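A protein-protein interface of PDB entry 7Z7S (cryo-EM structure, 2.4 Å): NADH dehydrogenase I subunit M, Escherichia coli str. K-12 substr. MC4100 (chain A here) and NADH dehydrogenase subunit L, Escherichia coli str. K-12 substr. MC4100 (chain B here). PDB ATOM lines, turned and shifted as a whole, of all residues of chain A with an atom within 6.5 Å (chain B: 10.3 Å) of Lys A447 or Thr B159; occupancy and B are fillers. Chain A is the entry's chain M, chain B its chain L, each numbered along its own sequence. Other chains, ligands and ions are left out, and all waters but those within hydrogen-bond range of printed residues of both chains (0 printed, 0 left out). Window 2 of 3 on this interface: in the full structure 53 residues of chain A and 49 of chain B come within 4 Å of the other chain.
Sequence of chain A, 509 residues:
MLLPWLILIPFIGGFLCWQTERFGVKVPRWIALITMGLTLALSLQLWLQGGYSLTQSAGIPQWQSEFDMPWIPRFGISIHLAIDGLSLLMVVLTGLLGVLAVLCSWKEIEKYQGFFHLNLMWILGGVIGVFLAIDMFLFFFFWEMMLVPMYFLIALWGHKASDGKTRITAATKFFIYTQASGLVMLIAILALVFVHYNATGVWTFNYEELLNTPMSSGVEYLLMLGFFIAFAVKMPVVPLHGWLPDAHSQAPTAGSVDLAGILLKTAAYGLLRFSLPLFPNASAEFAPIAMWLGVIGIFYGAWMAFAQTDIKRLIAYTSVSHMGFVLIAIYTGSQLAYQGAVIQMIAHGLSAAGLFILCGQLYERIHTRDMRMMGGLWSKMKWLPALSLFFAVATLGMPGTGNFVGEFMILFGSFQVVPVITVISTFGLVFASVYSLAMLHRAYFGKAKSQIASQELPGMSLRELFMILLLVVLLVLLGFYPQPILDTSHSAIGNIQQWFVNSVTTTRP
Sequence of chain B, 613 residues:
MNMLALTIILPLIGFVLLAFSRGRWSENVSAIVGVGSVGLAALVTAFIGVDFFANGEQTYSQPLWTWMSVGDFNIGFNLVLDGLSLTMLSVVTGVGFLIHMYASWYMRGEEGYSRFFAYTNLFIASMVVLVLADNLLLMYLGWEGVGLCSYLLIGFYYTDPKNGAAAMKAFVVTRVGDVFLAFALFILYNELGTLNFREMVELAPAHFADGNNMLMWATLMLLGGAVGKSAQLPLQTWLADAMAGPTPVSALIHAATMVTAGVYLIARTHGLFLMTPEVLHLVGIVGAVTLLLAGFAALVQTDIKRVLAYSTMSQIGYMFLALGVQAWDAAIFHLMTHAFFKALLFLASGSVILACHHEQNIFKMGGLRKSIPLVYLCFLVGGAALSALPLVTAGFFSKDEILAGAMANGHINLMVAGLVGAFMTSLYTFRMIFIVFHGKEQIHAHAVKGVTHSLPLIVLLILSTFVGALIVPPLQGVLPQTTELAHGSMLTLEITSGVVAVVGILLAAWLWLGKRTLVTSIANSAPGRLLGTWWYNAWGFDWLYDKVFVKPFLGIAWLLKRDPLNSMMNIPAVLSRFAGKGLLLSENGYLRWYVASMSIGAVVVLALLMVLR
O of Tyr B158 is in hydrogen-bond range of N of Gly A446, 2.8 Å away.
Of the 10 printed residues of chain A, 4 touch a printed residue of chain B. Printed residues of chain A that touch a printed residue of chain B: Ser A379, Phe A445, Gly A446 and Lys A447.
Among the printed residues, merely in contact across the chains: Ser A379 with Tyr B158, Lys A447 with Thr B159, Gly A446 with Thr B159 and Phe A445 with Tyr B158.
OG of Ser A379 sits at hydrogen-bond distance from O of Gly A376 (3.1 Å). The backbone carbonyl oxygen (O) of Phe A445 is in hydrogen-bond range of the backbone NH (N) of Gly A376 (3.4 Å). OH of Tyr B158 sits at hydrogen-bond distance from OE2 of Glu B111.
Of chain B, only Thr B159 (3.4 Å) comes within 4 Å of Lys A447. Of chain A, only Gly A446 (3.5 Å) and Lys A447 (3.4 Å) come within 4 Å of Thr B159. Printed residues of chain B within 4 Å of Gly A446: Tyr B158 (2.8 Å) and Thr B159 (3.5 Å). No residue of chain B comes within 4 Å of Ala A448. Of the printed residues of chain B, Phe A445 touches Tyr B158. Of the printed residues of chain B, Ser A379 touches Tyr B158. Of the printed residues of chain A, Tyr B158 touches Ser A379 (3.3 Å), Phe A445 (3.6 Å) and Gly A446 (2.8 Å). Gly B164 touches none of the printed residues of chain A. Arg B115 touches none of the printed residues of chain A.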
ATOM      1  N   MET A 374      10.028  14.302   1.531  1.00  0.00           N
ATOM      2  CA  MET A 374       9.967  14.996   0.254  1.00  0.00           C
ATOM      3  C   MET A 374      11.114  15.986   0.176  1.00  0.00           C
ATOM      4  O   MET A 374      11.365  16.723   1.132  1.00  0.00           O
ATOM      5  CB  MET A 374       8.630  15.718   0.073  1.00  0.00           C
ATOM      6  CG  MET A 374       8.061  16.320   1.332  1.00  0.00           C
ATOM      7  SD  MET A 374       6.684  17.423   0.994  1.00  0.00           S
ATOM      8  CE  MET A 374       5.663  17.165   2.435  1.00  0.00           C
ATOM      9  N   GLY A 375      11.815  15.991  -0.950  1.00  0.00           N
ATOM     10  CA  GLY A 375      12.898  16.925  -1.163  1.00  0.00           C
ATOM     11  C   GLY A 375      13.230  17.061  -2.630  1.00  0.00           C
ATOM     12  O   GLY A 375      13.131  16.090  -3.381  1.00  0.00           O
ATOM     13  N   GLY A 376      13.625  18.257  -3.051  1.00  0.00           N
ATOM     14  CA  GLY A 376      13.937  18.487  -4.451  1.00  0.00           C
ATOM     15  C   GLY A 376      12.756  18.299  -5.376  1.00  0.00           C
ATOM     16  O   GLY A 376      12.917  17.777  -6.485  1.00  0.00           O
ATOM     17  N   SER A 379      12.065  19.786  -9.432  1.00  0.00           N
ATOM     18  CA  SER A 379      12.352  19.091 -10.678  1.00  0.00           C
ATOM     19  C   SER A 379      11.348  17.998 -10.999  1.00  0.00           C
ATOM     20  O   SER A 379      11.416  17.424 -12.090  1.00  0.00           O
ATOM     21  CB  SER A 379      13.753  18.486 -10.619  1.00  0.00           C
ATOM     22  OG  SER A 379      13.958  17.832  -9.382  1.00  0.00           O
ATOM     23  N   PHE A 445      13.229  22.044  -2.472  1.00  0.00           N
ATOM     24  CA  PHE A 445      14.611  22.262  -2.859  1.00  0.00           C
ATOM     25  C   PHE A 445      15.496  21.209  -2.214  1.00  0.00           C
ATOM     26  O   PHE A 445      15.143  20.607  -1.197  1.00  0.00           O
ATOM     27  CB  PHE A 445      15.083  23.664  -2.464  1.00  0.00           C
ATOM     28  CG  PHE A 445      14.331  24.764  -3.141  1.00  0.00           C
ATOM     29  CD1 PHE A 445      13.984  24.662  -4.474  1.00  0.00           C
ATOM     30  CD2 PHE A 445      13.961  25.897  -2.444  1.00  0.00           C
ATOM     31  CE1 PHE A 445      13.292  25.670  -5.101  1.00  0.00           C
ATOM     32  CE2 PHE A 445      13.264  26.908  -3.065  1.00  0.00           C
ATOM     33  CZ  PHE A 445      12.929  26.794  -4.396  1.00  0.00           C
ATOM     34  N   GLY A 446      16.652  20.982  -2.827  1.00  0.00           N
ATOM     35  CA  GLY A 446      17.591  20.008  -2.313  1.00  0.00           C
ATOM     36  C   GLY A 446      17.558  18.706  -3.079  1.00  0.00           C
ATOM     37  O   GLY A 446      17.250  18.683  -4.272  1.00  0.00           O
ATOM     38  N   LYS A 447      17.881  17.615  -2.397  1.00  0.00           N
ATOM     39  CA  LYS A 447      17.857  16.282  -2.974  1.00  0.00           C
ATOM     40  C   LYS A 447      16.686  15.500  -2.399  1.00  0.00           C
ATOM     41  O   LYS A 447      16.181  15.806  -1.318  1.00  0.00           O
ATOM     42  CB  LYS A 447      19.167  15.543  -2.689  1.00  0.00           C
ATOM     43  CG  LYS A 447      20.340  16.018  -3.518  1.00  0.00           C
ATOM     44  CD  LYS A 447      20.258  15.506  -4.937  1.00  0.00           C
ATOM     45  CE  LYS A 447      21.628  15.073  -5.428  1.00  0.00           C
ATOM     46  NZ  LYS A 447      22.680  16.060  -5.061  1.00  0.00           N
ATOM     47  N   ALA A 448      16.262  14.477  -3.138  1.00  0.00           N
ATOM     48  CA  ALA A 448      15.159  13.639  -2.689  1.00  0.00           C
ATOM     49  C   ALA A 448      15.575  12.824  -1.474  1.00  0.00           C
ATOM     50  O   ALA A 448      16.637  12.195  -1.466  1.00  0.00           O
ATOM     51  CB  ALA A 448      14.703  12.717  -3.815  1.00  0.00           C
ATOM     52  N   LYS A 449      14.741  12.843  -0.441  1.00  0.00           N
ATOM     53  CA  LYS A 449      15.028  12.140   0.799  1.00  0.00           C
ATOM     54  C   LYS A 449      14.296  10.812   0.915  1.00  0.00           C
ATOM     55  O   LYS A 449      14.418  10.142   1.944  1.00  0.00           O
ATOM     56  CB  LYS A 449      14.686  13.031   1.994  1.00  0.00           C
ATOM     57  CG  LYS A 449      15.693  14.135   2.238  1.00  0.00           C
ATOM     58  CD  LYS A 449      15.175  15.139   3.247  1.00  0.00           C
ATOM     59  CE  LYS A 449      14.219  16.125   2.608  1.00  0.00           C
ATOM     60  NZ  LYS A 449      13.829  17.207   3.550  1.00  0.00           N
ATOM     61  N   SER A 450      13.546  10.416  -0.108  1.00  0.00           N
ATOM     62  CA  SER A 450      12.857   9.132  -0.123  1.00  0.00           C
ATOM     63  C   SER A 450      12.683   8.702  -1.574  1.00  0.00           C
ATOM     64  O   SER A 450      13.236   9.313  -2.492  1.00  0.00           O
ATOM     65  CB  SER A 450      11.516   9.217   0.615  1.00  0.00           C
ATOM     66  OG  SER A 450      10.594  10.020  -0.098  1.00  0.00           O
ATOM     67  N   GLU B 110      21.833  24.598 -19.411  1.00  0.00           N
ATOM     68  CA  GLU B 110      21.555  24.537 -17.985  1.00  0.00           C
ATOM     69  C   GLU B 110      20.060  24.392 -17.762  1.00  0.00           C
ATOM     70  O   GLU B 110      19.256  24.965 -18.502  1.00  0.00           O
ATOM     71  CB  GLU B 110      22.062  25.785 -17.261  1.00  0.00           C
ATOM     72  CG  GLU B 110      23.568  25.928 -17.252  1.00  0.00           C
ATOM     73  CD  GLU B 110      24.188  25.445 -15.962  1.00  0.00           C
ATOM     74  OE1 GLU B 110      23.552  24.627 -15.266  1.00  0.00           O
ATOM     75  OE2 GLU B 110      25.311  25.885 -15.645  1.00  0.00           O
ATOM     76  N   GLU B 111      19.695  23.614 -16.749  1.00  0.00           N
ATOM     77  CA  GLU B 111      18.308  23.564 -16.315  1.00  0.00           C
ATOM     78  C   GLU B 111      17.922  24.891 -15.675  1.00  0.00           C
ATOM     79  O   GLU B 111      18.694  25.480 -14.917  1.00  0.00           O
ATOM     80  CB  GLU B 111      18.100  22.416 -15.327  1.00  0.00           C
ATOM     81  CG  GLU B 111      16.648  21.976 -15.160  1.00  0.00           C
ATOM     82  CD  GLU B 111      15.890  22.803 -14.129  1.00  0.00           C
ATOM     83  OE1 GLU B 111      14.750  23.225 -14.420  1.00  0.00           O
ATOM     84  OE2 GLU B 111      16.435  23.032 -13.029  1.00  0.00           O
ATOM     85  N   GLY B 112      16.715  25.355 -15.979  1.00  0.00           N
ATOM     86  CA  GLY B 112      16.257  26.616 -15.435  1.00  0.00           C
ATOM     87  C   GLY B 112      16.821  27.834 -16.123  1.00  0.00           C
ATOM     88  O   GLY B 112      16.964  28.880 -15.485  1.00  0.00           O
ATOM     89  N   ARG B 115      14.085  30.130 -16.183  1.00  0.00           N
ATOM     90  CA  ARG B 115      13.884  30.506 -14.786  1.00  0.00           C
ATOM     91  C   ARG B 115      14.946  31.495 -14.330  1.00  0.00           C
ATOM     92  O   ARG B 115      14.644  32.454 -13.606  1.00  0.00           O
ATOM     93  CB  ARG B 115      13.888  29.264 -13.899  1.00  0.00           C
ATOM     94  CG  ARG B 115      13.791  29.553 -12.416  1.00  0.00           C
ATOM     95  CD  ARG B 115      13.586  28.290 -11.618  1.00  0.00           C
ATOM     96  NE  ARG B 115      14.459  27.216 -12.073  1.00  0.00           N
ATOM     97  CZ  ARG B 115      15.541  26.808 -11.428  1.00  0.00           C
ATOM     98  NH1 ARG B 115      15.912  27.357 -10.283  1.00  0.00           N
ATOM     99  NH2 ARG B 115      16.269  25.824 -11.944  1.00  0.00           N
ATOM    100  N   LEU B 152      16.357  34.203  -4.532  1.00  0.00           N
ATOM    101  CA  LEU B 152      15.994  33.235  -5.565  1.00  0.00           C
ATOM    102  C   LEU B 152      17.169  32.923  -6.485  1.00  0.00           C
ATOM    103  O   LEU B 152      17.308  31.790  -6.959  1.00  0.00           O
ATOM    104  CB  LEU B 152      14.814  33.754  -6.382  1.00  0.00           C
ATOM    105  CG  LEU B 152      13.430  33.698  -5.740  1.00  0.00           C
ATOM    106  CD1 LEU B 152      12.433  34.457  -6.586  1.00  0.00           C
ATOM    107  CD2 LEU B 152      12.989  32.264  -5.545  1.00  0.00           C
ATOM    108  N   ILE B 154      20.553  33.372  -5.731  1.00  0.00           N
ATOM    109  CA  ILE B 154      21.711  32.813  -5.042  1.00  0.00           C
ATOM    110  C   ILE B 154      21.582  31.299  -4.934  1.00  0.00           C
ATOM    111  O   ILE B 154      22.518  30.554  -5.244  1.00  0.00           O
ATOM    112  CB  ILE B 154      21.880  33.475  -3.664  1.00  0.00           C
ATOM    113  CG1 ILE B 154      22.519  34.849  -3.821  1.00  0.00           C
ATOM    114  CG2 ILE B 154      22.715  32.610  -2.747  1.00  0.00           C
ATOM    115  CD1 ILE B 154      22.376  35.719  -2.599  1.00  0.00           C
ATOM    116  N   GLY B 155      20.414  30.822  -4.524  1.00  0.00           N
ATOM    117  CA  GLY B 155      20.172  29.398  -4.470  1.00  0.00           C
ATOM    118  C   GLY B 155      19.595  28.871  -5.763  1.00  0.00           C
ATOM    119  O   GLY B 155      18.641  28.091  -5.746  1.00  0.00           O
ATOM    120  N   PHE B 156      20.161  29.303  -6.892  1.00  0.00           N
ATOM    121  CA  PHE B 156      19.648  28.888  -8.191  1.00  0.00           C
ATOM    122  C   PHE B 156      19.885  27.404  -8.429  1.00  0.00           C
ATOM    123  O   PHE B 156      19.000  26.700  -8.925  1.00  0.00           O
ATOM    124  CB  PHE B 156      20.291  29.714  -9.301  1.00  0.00           C
ATOM    125  CG  PHE B 156      19.860  29.305 -10.672  1.00  0.00           C
ATOM    126  CD1 PHE B 156      18.602  29.636 -11.140  1.00  0.00           C
ATOM    127  CD2 PHE B 156      20.703  28.573 -11.487  1.00  0.00           C
ATOM    128  CE1 PHE B 156      18.200  29.252 -12.394  1.00  0.00           C
ATOM    129  CE2 PHE B 156      20.301  28.185 -12.739  1.00  0.00           C
ATOM    130  CZ  PHE B 156      19.053  28.525 -13.192  1.00  0.00           C
ATOM    131  N   TYR B 157      21.072  26.914  -8.089  1.00  0.00           N
ATOM    132  CA  TYR B 157      21.354  25.483  -8.121  1.00  0.00           C
ATOM    133  C   TYR B 157      20.795  24.893  -6.833  1.00  0.00           C
ATOM    134  O   TYR B 157      21.505  24.646  -5.856  1.00  0.00           O
ATOM    135  CB  TYR B 157      22.845  25.229  -8.267  1.00  0.00           C
ATOM    136  CG  TYR B 157      23.443  25.823  -9.513  1.00  0.00           C
ATOM    137  CD1 TYR B 157      22.824  25.666 -10.741  1.00  0.00           C
ATOM    138  CD2 TYR B 157      24.624  26.547  -9.460  1.00  0.00           C
ATOM    139  CE1 TYR B 157      23.367  26.208 -11.884  1.00  0.00           C
ATOM    140  CE2 TYR B 157      25.174  27.091 -10.597  1.00  0.00           C
ATOM    141  CZ  TYR B 157      24.541  26.918 -11.807  1.00  0.00           C
ATOM    142  OH  TYR B 157      25.084  27.459 -12.947  1.00  0.00           O
ATOM    143  N   TYR B 158      19.480  24.679  -6.838  1.00  0.00           N
ATOM    144  CA  TYR B 158      18.759  24.255  -5.648  1.00  0.00           C
ATOM    145  C   TYR B 158      19.066  22.822  -5.244  1.00  0.00           C
ATOM    146  O   TYR B 158      18.706  22.429  -4.132  1.00  0.00           O
ATOM    147  CB  TYR B 158      17.255  24.415  -5.864  1.00  0.00           C
ATOM    148  CG  TYR B 158      16.694  23.625  -7.021  1.00  0.00           C
ATOM    149  CD1 TYR B 158      16.657  24.162  -8.297  1.00  0.00           C
ATOM    150  CD2 TYR B 158      16.184  22.346  -6.835  1.00  0.00           C
ATOM    151  CE1 TYR B 158      16.145  23.451  -9.353  1.00  0.00           C
ATOM    152  CE2 TYR B 158      15.673  21.627  -7.887  1.00  0.00           C
ATOM    153  CZ  TYR B 158      15.654  22.184  -9.143  1.00  0.00           C
ATOM    154  OH  TYR B 158      15.143  21.475 -10.200  1.00  0.00           O
ATOM    155  N   THR B 159      19.701  22.042  -6.121  1.00  0.00           N
ATOM    156  CA  THR B 159      20.030  20.657  -5.807  1.00  0.00           C
ATOM    157  C   THR B 159      21.037  20.568  -4.664  1.00  0.00           C
ATOM    158  O   THR B 159      20.884  19.747  -3.754  1.00  0.00           O
ATOM    159  CB  THR B 159      20.557  19.971  -7.066  1.00  0.00           C
ATOM    160  OG1 THR B 159      19.494  19.857  -8.018  1.00  0.00           O
ATOM    161  CG2 THR B 159      21.092  18.592  -6.758  1.00  0.00           C
ATOM    162  N   ASP B 160      22.057  21.414  -4.682  1.00  0.00           N
ATOM    163  CA  ASP B 160      23.026  21.445  -3.596  1.00  0.00           C
ATOM    164  C   ASP B 160      22.395  22.158  -2.406  1.00  0.00           C
ATOM    165  O   ASP B 160      21.966  23.309  -2.548  1.00  0.00           O
ATOM    166  CB  ASP B 160      24.297  22.155  -4.052  1.00  0.00           C
ATOM    167  CG  ASP B 160      25.462  22.018  -3.070  1.00  0.00           C
ATOM    168  OD1 ASP B 160      26.608  22.259  -3.503  1.00  0.00           O
ATOM    169  OD2 ASP B 160      25.269  21.662  -1.889  1.00  0.00           O
ATOM    170  N   PRO B 161      22.296  21.518  -1.236  1.00  0.00           N
ATOM    171  CA  PRO B 161      21.683  22.192  -0.080  1.00  0.00           C
ATOM    172  C   PRO B 161      22.485  23.363   0.461  1.00  0.00           C
ATOM    173  O   PRO B 161      21.911  24.216   1.147  1.00  0.00           O
ATOM    174  CB  PRO B 161      21.571  21.068   0.961  1.00  0.00           C
ATOM    175  CG  PRO B 161      21.634  19.808   0.170  1.00  0.00           C
ATOM    176  CD  PRO B 161      22.556  20.097  -0.966  1.00  0.00           C
ATOM    177  N   LYS B 162      23.787  23.438   0.180  1.00  0.00           N
ATOM    178  CA  LYS B 162      24.578  24.550   0.695  1.00  0.00           C
ATOM    179  C   LYS B 162      24.272  25.847  -0.041  1.00  0.00           C
ATOM    180  O   LYS B 162      24.342  26.925   0.561  1.00  0.00           O
ATOM    181  CB  LYS B 162      26.070  24.214   0.623  1.00  0.00           C
ATOM    182  CG  LYS B 162      26.636  23.036   1.495  1.00  0.00           C
ATOM    183  CD  LYS B 162      25.867  22.456   2.736  1.00  0.00           C
ATOM    184  CE  LYS B 162      25.428  23.445   3.844  1.00  0.00           C
ATOM    185  NZ  LYS B 162      24.381  22.869   4.734  1.00  0.00           N
ATOM    186  N   ASN B 163      23.922  25.764  -1.325  1.00  0.00           N
ATOM    187  CA  ASN B 163      23.433  26.941  -2.037  1.00  0.00           C
ATOM    188  C   ASN B 163      22.133  27.446  -1.427  1.00  0.00           C
ATOM    189  O   ASN B 163      21.930  28.659  -1.288  1.00  0.00           O
ATOM    190  CB  ASN B 163      23.239  26.623  -3.518  1.00  0.00           C
ATOM    191  CG  ASN B 163      24.497  26.102  -4.170  1.00  0.00           C
ATOM    192  OD1 ASN B 163      24.442  25.286  -5.085  1.00  0.00           O
ATOM    193  ND2 ASN B 163      25.643  26.578  -3.707  1.00  0.00           N
ATOM    194  N   GLY B 164      21.251  26.527  -1.038  1.00  0.00           N
ATOM    195  CA  GLY B 164      20.025  26.924  -0.373  1.00  0.00           C
ATOM    196  C   GLY B 164      20.263  27.536   0.993  1.00  0.00           C
ATOM    197  O   GLY B 164      19.584  28.491   1.379  1.00  0.00           O
ATOM    198  N   ALA B 165      21.228  26.997   1.742  1.00  0.00           N
ATOM    199  CA  ALA B 165      21.576  27.581   3.034  1.00  0.00           C
ATOM    200  C   ALA B 165      22.165  28.976   2.872  1.00  0.00           C
ATOM    201  O   ALA B 165      21.875  29.876   3.669  1.00  0.00           O
ATOM    202  CB  ALA B 165      22.549  26.671   3.776  1.00  0.00           C
ATOM    203  N   ALA B 244      27.676  32.074  -3.409  1.00  0.00           N
ATOM    204  CA  ALA B 244      27.797  30.711  -3.899  1.00  0.00           C
ATOM    205  C   ALA B 244      26.838  30.401  -5.044  1.00  0.00           C
ATOM    206  O   ALA B 244      26.657  29.229  -5.381  1.00  0.00           O
ATOM    207  CB  ALA B 244      27.569  29.723  -2.755  1.00  0.00           C
